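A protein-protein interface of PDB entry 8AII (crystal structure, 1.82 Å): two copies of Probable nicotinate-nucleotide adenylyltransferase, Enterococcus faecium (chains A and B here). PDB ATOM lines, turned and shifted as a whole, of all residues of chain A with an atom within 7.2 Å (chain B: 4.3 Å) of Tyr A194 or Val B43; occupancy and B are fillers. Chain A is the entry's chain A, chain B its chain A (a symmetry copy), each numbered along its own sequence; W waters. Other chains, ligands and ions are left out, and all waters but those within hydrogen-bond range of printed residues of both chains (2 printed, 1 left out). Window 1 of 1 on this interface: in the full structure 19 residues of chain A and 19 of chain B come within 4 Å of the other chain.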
ATOM      1  N   HIS A  38      14.475   8.558  20.602  1.00  0.00           N
ATOM      2  CA  HIS A  38      13.648   8.497  19.394  1.00  0.00           C
ATOM      3  C   HIS A  38      13.973   9.666  18.473  1.00  0.00           C
ATOM      4  O   HIS A  38      14.822  10.506  18.781  1.00  0.00           O
ATOM      5  CB  HIS A  38      12.161   8.496  19.735  1.00  0.00           C
ATOM      6  CG  HIS A  38      11.758   9.629  20.622  1.00  0.00           C
ATOM      7  ND1 HIS A  38      11.832  10.946  20.223  1.00  0.00           N
ATOM      8  CD2 HIS A  38      11.299   9.643  21.897  1.00  0.00           C
ATOM      9  CE1 HIS A  38      11.427  11.722  21.213  1.00  0.00           C
ATOM     10  NE2 HIS A  38      11.101  10.956  22.241  1.00  0.00           N
ATOM     11  N   LEU A  39      13.270   9.720  17.327  1.00  0.00           N
ATOM     12  CA  LEU A  39      13.665  10.658  16.278  1.00  0.00           C
ATOM     13  C   LEU A  39      13.625  12.105  16.745  1.00  0.00           C
ATOM     14  O   LEU A  39      14.444  12.918  16.310  1.00  0.00           O
ATOM     15  CB  LEU A  39      12.779  10.498  15.042  1.00  0.00           C
ATOM     16  CG  LEU A  39      13.468   9.726  13.922  1.00  0.00           C
ATOM     17  CD1 LEU A  39      14.472  10.649  13.230  1.00  0.00           C
ATOM     18  CD2 LEU A  39      14.146   8.449  14.446  1.00  0.00           C
ATOM     19  N   ALA A  40      12.668  12.461  17.599  1.00  0.00           N
ATOM     20  CA  ALA A  40      12.572  13.864  17.995  1.00  0.00           C
ATOM     21  C   ALA A  40      13.796  14.296  18.797  1.00  0.00           C
ATOM     22  O   ALA A  40      14.280  15.425  18.638  1.00  0.00           O
ATOM     23  CB  ALA A  40      11.288  14.107  18.788  1.00  0.00           C
ATOM     24  N   ILE A 177       6.759  13.536  18.944  1.00  0.00           N
ATOM     25  CA  ILE A 177       7.042  12.194  19.436  1.00  0.00           C
ATOM     26  C   ILE A 177       7.509  12.331  20.880  1.00  0.00           C
ATOM     27  O   ILE A 177       8.235  13.274  21.210  1.00  0.00           O
ATOM     28  CB  ILE A 177       8.136  11.498  18.593  1.00  0.00           C
ATOM     29  CG1 ILE A 177       7.745  11.405  17.114  1.00  0.00           C
ATOM     30  CG2 ILE A 177       8.487  10.116  19.162  1.00  0.00           C
ATOM     31  CD1 ILE A 177       8.911  10.922  16.243  1.00  0.00           C
ATOM     32  N   SER A 191       3.215   0.112  15.079  1.00  0.00           N
ATOM     33  CA  SER A 191       4.499   0.378  14.441  1.00  0.00           C
ATOM     34  C   SER A 191       5.175   1.583  15.060  1.00  0.00           C
ATOM     35  O   SER A 191       4.523   2.578  15.386  1.00  0.00           O
ATOM     36  CB  SER A 191       4.322   0.620  12.940  1.00  0.00           C
ATOM     37  OG  SER A 191       5.568   0.969  12.344  1.00  0.00           O
ATOM     38  N   ILE A 192       6.500   1.494  15.194  1.00  0.00           N
ATOM     39  CA  ILE A 192       7.350   2.604  15.592  1.00  0.00           C
ATOM     40  C   ILE A 192       8.423   2.886  14.554  1.00  0.00           C
ATOM     41  O   ILE A 192       9.331   3.666  14.810  1.00  0.00           O
ATOM     42  CB  ILE A 192       7.977   2.368  16.981  1.00  0.00           C
ATOM     43  CG1 ILE A 192       9.048   1.272  16.935  1.00  0.00           C
ATOM     44  CG2 ILE A 192       6.893   2.017  17.998  1.00  0.00           C
ATOM     45  CD1 ILE A 192       9.837   1.130  18.256  1.00  0.00           C
ATOM     46  N   ARG A 193       8.324   2.270  13.372  1.00  0.00           N
ATOM     47  CA  ARG A 193       9.337   2.493  12.350  1.00  0.00           C
ATOM     48  C   ARG A 193       9.365   3.959  11.948  1.00  0.00           C
ATOM     49  O   ARG A 193       8.317   4.592  11.820  1.00  0.00           O
ATOM     50  CB  ARG A 193       9.062   1.632  11.122  1.00  0.00           C
ATOM     51  CG  ARG A 193      10.174   1.724  10.101  1.00  0.00           C
ATOM     52  CD  ARG A 193      10.060   0.584   9.130  1.00  0.00           C
ATOM     53  NE  ARG A 193      11.278   0.384   8.354  1.00  0.00           N
ATOM     54  CZ  ARG A 193      11.539  -0.737   7.690  1.00  0.00           C
ATOM     55  NH1 ARG A 193      10.673  -1.737   7.736  1.00  0.00           N
ATOM     56  NH2 ARG A 193      12.664  -0.861   6.998  1.00  0.00           N
ATOM     57  N   TYR A 194      10.575   4.476  11.726  1.00  0.00           N
ATOM     58  CA  TYR A 194      10.868   5.875  11.400  1.00  0.00           C
ATOM     59  C   TYR A 194      10.706   6.803  12.613  1.00  0.00           C
ATOM     60  O   TYR A 194      11.363   7.843  12.681  1.00  0.00           O
ATOM     61  CB  TYR A 194      10.003   6.362  10.217  1.00  0.00           C
ATOM     62  CG  TYR A 194      10.109   5.490   8.971  1.00  0.00           C
ATOM     63  CD1 TYR A 194      11.309   5.391   8.250  1.00  0.00           C
ATOM     64  CD2 TYR A 194       9.024   4.770   8.527  1.00  0.00           C
ATOM     65  CE1 TYR A 194      11.398   4.575   7.098  1.00  0.00           C
ATOM     66  CE2 TYR A 194       9.095   3.950   7.365  1.00  0.00           C
ATOM     67  CZ  TYR A 194      10.292   3.858   6.673  1.00  0.00           C
ATOM     68  OH  TYR A 194      10.360   3.056   5.552  1.00  0.00           O
ATOM     69  N   LEU A 195       9.833   6.467  13.571  1.00  0.00           N
ATOM     70  CA  LEU A 195       9.783   7.245  14.811  1.00  0.00           C
ATOM     71  C   LEU A 195      10.983   6.976  15.703  1.00  0.00           C
ATOM     72  O   LEU A 195      11.281   7.781  16.598  1.00  0.00           O
ATOM     73  CB  LEU A 195       8.514   6.920  15.595  1.00  0.00           C
ATOM     74  CG  LEU A 195       7.205   7.032  14.828  1.00  0.00           C
ATOM     75  CD1 LEU A 195       6.088   6.488  15.681  1.00  0.00           C
ATOM     76  CD2 LEU A 195       6.943   8.478  14.449  1.00  0.00           C
ATOM     77  N   VAL A 196      11.663   5.858  15.487  1.00  0.00           N
ATOM     78  CA  VAL A 196      12.746   5.366  16.337  1.00  0.00           C
ATOM     79  C   VAL A 196      13.796   4.789  15.397  1.00  0.00           C
ATOM     80  O   VAL A 196      13.428   4.080  14.444  1.00  0.00           O
ATOM     81  CB  VAL A 196      12.237   4.286  17.313  1.00  0.00           C
ATOM     82  CG1 VAL A 196      13.375   3.728  18.141  1.00  0.00           C
ATOM     83  CG2 VAL A 196      11.117   4.807  18.205  1.00  0.00           C
ATOM     84  N   PRO A 197      15.089   5.031  15.619  1.00  0.00           N
ATOM     85  CA  PRO A 197      16.101   4.514  14.687  1.00  0.00           C
ATOM     86  C   PRO A 197      16.074   2.998  14.586  1.00  0.00           C
ATOM     87  O   PRO A 197      15.755   2.290  15.550  1.00  0.00           O
ATOM     88  CB  PRO A 197      17.424   5.013  15.293  1.00  0.00           C
ATOM     89  CG  PRO A 197      17.036   6.257  16.028  1.00  0.00           C
ATOM     90  CD  PRO A 197      15.675   5.951  16.608  1.00  0.00           C
ATOM     91  N   ASP A 198      16.440   2.505  13.396  1.00  0.00           N
ATOM     92  CA  ASP A 198      16.332   1.079  13.105  1.00  0.00           C
ATOM     93  C   ASP A 198      17.146   0.253  14.091  1.00  0.00           C
ATOM     94  O   ASP A 198      16.678  -0.786  14.573  1.00  0.00           O
ATOM     95  CB  ASP A 198      16.792   0.789  11.669  1.00  0.00           C
ATOM     96  CG  ASP A 198      15.740   1.155  10.613  1.00  0.00           C
ATOM     97  OD1 ASP A 198      14.536   1.256  10.937  1.00  0.00           O
ATOM     98  OD2 ASP A 198      16.127   1.317   9.438  1.00  0.00           O
ATOM     99  N   ILE A 201      15.154   0.132  17.344  1.00  0.00           N
ATOM    100  CA  ILE A 201      14.033  -0.811  17.237  1.00  0.00           C
ATOM    101  C   ILE A 201      14.529  -2.245  17.401  1.00  0.00           C
ATOM    102  O   ILE A 201      13.941  -3.050  18.137  1.00  0.00           O
ATOM    103  CB  ILE A 201      13.289  -0.637  15.896  1.00  0.00           C
ATOM    104  CG1 ILE A 201      12.532   0.692  15.840  1.00  0.00           C
ATOM    105  CG2 ILE A 201      12.305  -1.803  15.690  1.00  0.00           C
ATOM    106  CD1 ILE A 201      11.894   0.984  14.494  1.00  0.00           C
ATOM    107  N   LEU B  39      11.372  12.700   6.015  1.00  0.00           N
ATOM    108  CA  LEU B  39      10.915  11.821   7.090  1.00  0.00           C
ATOM    109  C   LEU B  39       9.406  11.864   7.276  1.00  0.00           C
ATOM    110  O   LEU B  39       8.797  10.850   7.622  1.00  0.00           O
ATOM    111  CB  LEU B  39      11.600  12.175   8.411  1.00  0.00           C
ATOM    112  CG  LEU B  39      12.721  11.205   8.769  1.00  0.00           C
ATOM    113  CD1 LEU B  39      12.106   9.910   9.297  1.00  0.00           C
ATOM    114  CD2 LEU B  39      13.646  10.940   7.570  1.00  0.00           C
ATOM    115  N   ALA B  40       8.785  13.026   7.085  1.00  0.00           N
ATOM    116  CA  ALA B  40       7.347  13.098   7.335  1.00  0.00           C
ATOM    117  C   ALA B  40       6.571  12.235   6.345  1.00  0.00           C
ATOM    118  O   ALA B  40       5.578  11.595   6.718  1.00  0.00           O
ATOM    119  CB  ALA B  40       6.869  14.548   7.285  1.00  0.00           C
ATOM    120  N   HIS B  41       7.025  12.176   5.085  1.00  0.00           N
ATOM    121  CA  HIS B  41       6.407  11.267   4.112  1.00  0.00           C
ATOM    122  C   HIS B  41       6.439   9.833   4.613  1.00  0.00           C
ATOM    123  O   HIS B  41       5.444   9.106   4.523  1.00  0.00           O
ATOM    124  CB  HIS B  41       7.130  11.340   2.763  1.00  0.00           C
ATOM    125  CG  HIS B  41       7.036  12.660   2.089  1.00  0.00           C
ATOM    126  ND1 HIS B  41       8.148  13.323   1.613  1.00  0.00           N
ATOM    127  CD2 HIS B  41       5.971  13.431   1.772  1.00  0.00           C
ATOM    128  CE1 HIS B  41       7.770  14.446   1.035  1.00  0.00           C
ATOM    129  NE2 HIS B  41       6.455  14.541   1.127  1.00  0.00           N
ATOM    130  N   LEU B  42       7.586   9.405   5.145  1.00  0.00           N
ATOM    131  CA  LEU B  42       7.735   8.019   5.571  1.00  0.00           C
ATOM    132  C   LEU B  42       6.904   7.707   6.805  1.00  0.00           C
ATOM    133  O   LEU B  42       6.308   6.624   6.899  1.00  0.00           O
ATOM    134  CB  LEU B  42       9.204   7.693   5.833  1.00  0.00           C
ATOM    135  CG  LEU B  42      10.136   7.778   4.632  1.00  0.00           C
ATOM    136  CD1 LEU B  42      11.605   7.597   5.049  1.00  0.00           C
ATOM    137  CD2 LEU B  42       9.730   6.746   3.574  1.00  0.00           C
ATOM    138  N   VAL B  43       6.901   8.610   7.785  1.00  0.00           N
ATOM    139  CA  VAL B  43       6.077   8.417   8.975  1.00  0.00           C
ATOM    140  C   VAL B  43       4.594   8.415   8.612  1.00  0.00           C
ATOM    141  O   VAL B  43       3.826   7.579   9.092  1.00  0.00           O
ATOM    142  CB  VAL B  43       6.379   9.500  10.015  1.00  0.00           C
ATOM    143  CG1 VAL B  43       5.283   9.487  11.117  1.00  0.00           C
ATOM    144  CG2 VAL B  43       7.798   9.284  10.610  1.00  0.00           C
ATOM    145  N   MET B  44       4.162   9.375   7.792  1.00  0.00           N
ATOM    146  CA  MET B  44       2.739   9.439   7.438  1.00  0.00           C
ATOM    147  C   MET B  44       2.297   8.163   6.732  1.00  0.00           C
ATOM    148  O   MET B  44       1.258   7.578   7.062  1.00  0.00           O
ATOM    149  CB  MET B  44       2.471  10.655   6.562  1.00  0.00           C
ATOM    150  CG  MET B  44       2.383  11.974   7.302  1.00  0.00           C
ATOM    151  SD  MET B  44       1.823  13.304   6.207  1.00  0.00           S
ATOM    152  CE  MET B  44       3.139  13.351   4.985  1.00  0.00           C
ATOM    153  N   ALA B  45       3.085   7.714   5.759  1.00  0.00           N
ATOM    154  CA  ALA B  45       2.723   6.530   4.997  1.00  0.00           C
ATOM    155  C   ALA B  45       2.737   5.294   5.878  1.00  0.00           C
ATOM    156  O   ALA B  45       1.760   4.538   5.918  1.00  0.00           O
ATOM    157  CB  ALA B  45       3.677   6.358   3.822  1.00  0.00           C
ATOM    158  N   GLU B  46       3.844   5.063   6.597  1.00  0.00           N
ATOM    159  CA  GLU B  46       3.916   3.867   7.430  1.00  0.00           C
ATOM    160  C   GLU B  46       2.855   3.868   8.519  1.00  0.00           C
ATOM    161  O   GLU B  46       2.200   2.844   8.751  1.00  0.00           O
ATOM    162  CB  GLU B  46       5.305   3.729   8.058  1.00  0.00           C
ATOM    163  CG  GLU B  46       5.459   2.443   8.843  1.00  0.00           C
ATOM    164  CD  GLU B  46       5.927   1.318   7.975  1.00  0.00           C
ATOM    165  OE1 GLU B  46       6.322   1.610   6.834  1.00  0.00           O
ATOM    166  OE2 GLU B  46       5.958   0.153   8.441  1.00  0.00           O
ATOM    167  N   GLN B  47       2.668   5.001   9.210  1.00  0.00           N
ATOM    168  CA  GLN B  47       1.746   5.011  10.346  1.00  0.00           C
ATOM    169  C   GLN B  47       0.295   4.857   9.876  1.00  0.00           C
ATOM    170  O   GLN B  47      -0.475   4.090  10.464  1.00  0.00           O
ATOM    171  CB  GLN B  47       1.888   6.301  11.138  1.00  0.00           C
ATOM    172  CG  GLN B  47       3.149   6.358  12.017  1.00  0.00           C
ATOM    173  CD  GLN B  47       2.970   5.577  13.308  1.00  0.00           C
ATOM    174  OE1 GLN B  47       2.149   5.932  14.162  1.00  0.00           O
ATOM    175  NE2 GLN B  47       3.716   4.496  13.445  1.00  0.00           N
ATOM    176  N   ASN B  90      12.071  -1.707   3.059  1.00  0.00           N
ATOM    177  CA  ASN B  90      10.783  -1.766   3.741  1.00  0.00           C
ATOM    178  C   ASN B  90       9.743  -2.232   2.738  1.00  0.00           C
ATOM    179  O   ASN B  90       9.205  -1.421   1.975  1.00  0.00           O
ATOM    180  CB  ASN B  90      10.421  -0.400   4.319  1.00  0.00           C
ATOM    181  CG  ASN B  90       9.118  -0.420   5.076  1.00  0.00           C
ATOM    182  OD1 ASN B  90       8.459  -1.450   5.149  1.00  0.00           O
ATOM    183  ND2 ASN B  90       8.737   0.723   5.646  1.00  0.00           N
ATOM    184  N   LEU B  93       6.372  -0.191   2.050  1.00  0.00           N
ATOM    185  CA  LEU B  93       6.268   1.075   1.338  1.00  0.00           C
ATOM    186  C   LEU B  93       6.861   0.902  -0.047  1.00  0.00           C
ATOM    187  O   LEU B  93       7.970   0.366  -0.189  1.00  0.00           O
ATOM    188  CB  LEU B  93       6.997   2.209   2.078  1.00  0.00           C
ATOM    189  CG  LEU B  93       6.513   2.607   3.470  1.00  0.00           C
ATOM    190  CD1 LEU B  93       7.382   3.728   3.928  1.00  0.00           C
ATOM    191  CD2 LEU B  93       5.081   3.082   3.423  1.00  0.00           C
ATOM    192  N   VAL B 172      -1.570  10.258  13.483  1.00  0.00           N
ATOM    193  CA  VAL B 172      -0.163  10.127  13.101  1.00  0.00           C
ATOM    194  C   VAL B 172       0.576  11.179  13.924  1.00  0.00           C
ATOM    195  O   VAL B 172       0.065  12.302  14.064  1.00  0.00           O
ATOM    196  CB  VAL B 172       0.034  10.321  11.585  1.00  0.00           C
ATOM    197  CG1 VAL B 172       1.506  10.407  11.217  1.00  0.00           C
ATOM    198  CG2 VAL B 172      -0.608   9.172  10.812  1.00  0.00           C
ATOM    199  N   ILE B 175       4.597  15.614  12.292  1.00  0.00           N
ATOM    200  CA  ILE B 175       5.965  15.818  11.808  1.00  0.00           C
ATOM    201  C   ILE B 175       5.922  17.018  10.873  1.00  0.00           C
ATOM    202  O   ILE B 175       5.506  16.892   9.716  1.00  0.00           O
ATOM    203  CB  ILE B 175       6.525  14.594  11.079  1.00  0.00           C
ATOM    204  CG1 ILE B 175       6.149  13.304  11.795  1.00  0.00           C
ATOM    205  CG2 ILE B 175       8.027  14.718  10.920  1.00  0.00           C
ATOM    206  CD1 ILE B 175       6.783  13.164  13.124  1.00  0.00           C
HETATM  207  O   HOH W   1       7.369  -1.759   7.501  1.00  0.00           O
HETATM  208  O   HOH W   2       5.598   3.938  11.955  1.00  0.00           O
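NE2 of Gln B47 lies within hydrogen-bond range of O of Ser A191, at 2.8 Å. The side-chain amide oxygen (OD1) of Asn B90 lies close to the guanidinium group (NH1) of Arg A193 (3.4 Å). The side-chain hydroxyl (OH) of Tyr A194 sits at hydrogen-bond distance from the side-chain amide nitrogen (ND2) of Asn B90, at 2.8 Å.
The backbone carbonyl oxygen of Leu A195 lies within hydrogen-bond range of the backbone NH of Leu A39 (2.9 Å). N of Arg A193 is in hydrogen-bond range of OG of Ser A191 (3.2 Å). OE1 of Glu B46 lies within hydrogen-bond range of ND2 of Asn B90, 2.8 Å away.
Ser A191 touches Glu B46. Tyr A194 touches Leu B42 (CE1 to CD1, 3.7 Å). CG2 of Val B43 touches CB of Tyr A194, 3.7 Å away. Tyr A194 touches Glu B46. Tyr A194 touches Leu B93. Leu A195 touches Val B43 (CD2 to CG1, 3.9 Å). Gln B47 touches Leu A195 (NE2 to CD1, 3.8 Å).
Of chain B, only Leu B42, Val B43, Glu B46, Asn B90 and Leu B93 come within 4 Å of Tyr A194. Asp A198 touches none of the printed residues of chain B. Printed residues of chain A within 4 Å of Leu B42: Tyr A194. Of chain A, only Tyr A194 (3.7 Å) and Leu A195 (3.9 Å) come within 4 Å of Val B43. Of the printed residues of chain A, Glu B46 touches Ser A191 and Tyr A194. Of the printed residues of chain A, Gln B47 touches Ser A191 and Leu A195. The nearest residue of chain B that does not touch Tyr A194 is Leu B39 (4.03 Å). The nearest residue of chain A that does not touch Val B43 is Arg A193 (4.9 Å). The nearest printed residue of chain A that does not touch Leu B42 is Arg A193 (5.7 Å).
Of the 13 printed residues of chain B, 6 touch a printed residue of chain A. Printed residues of chain B that touch a printed residue of chain A: Leu B42, Val B43, Glu B46, Gln B47, Asn B90 and Leu B93. Of the 13 printed residues of chain A, 4 touch a printed residue of chain B. Hydrophobic or aromatic side chains of chain A within 4 Å of the printed part of chain B: Tyr A194 and Leu A195. Among the printed residues, 10 pairs touch across the chains.
2 positions are printed for both chains.
Water W2 lies within hydrogen-bond range of NE2 of Gln B47, O of Arg A193 and OG of Ser A191. Water W1 lies within hydrogen-bond range of the side-chain carboxylate of Glu B46 (2.6 Å), the side-chain amide oxygen of Asn B90 (2.6 Å) and the guanidinium group of Arg A193 (3.3 Å).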
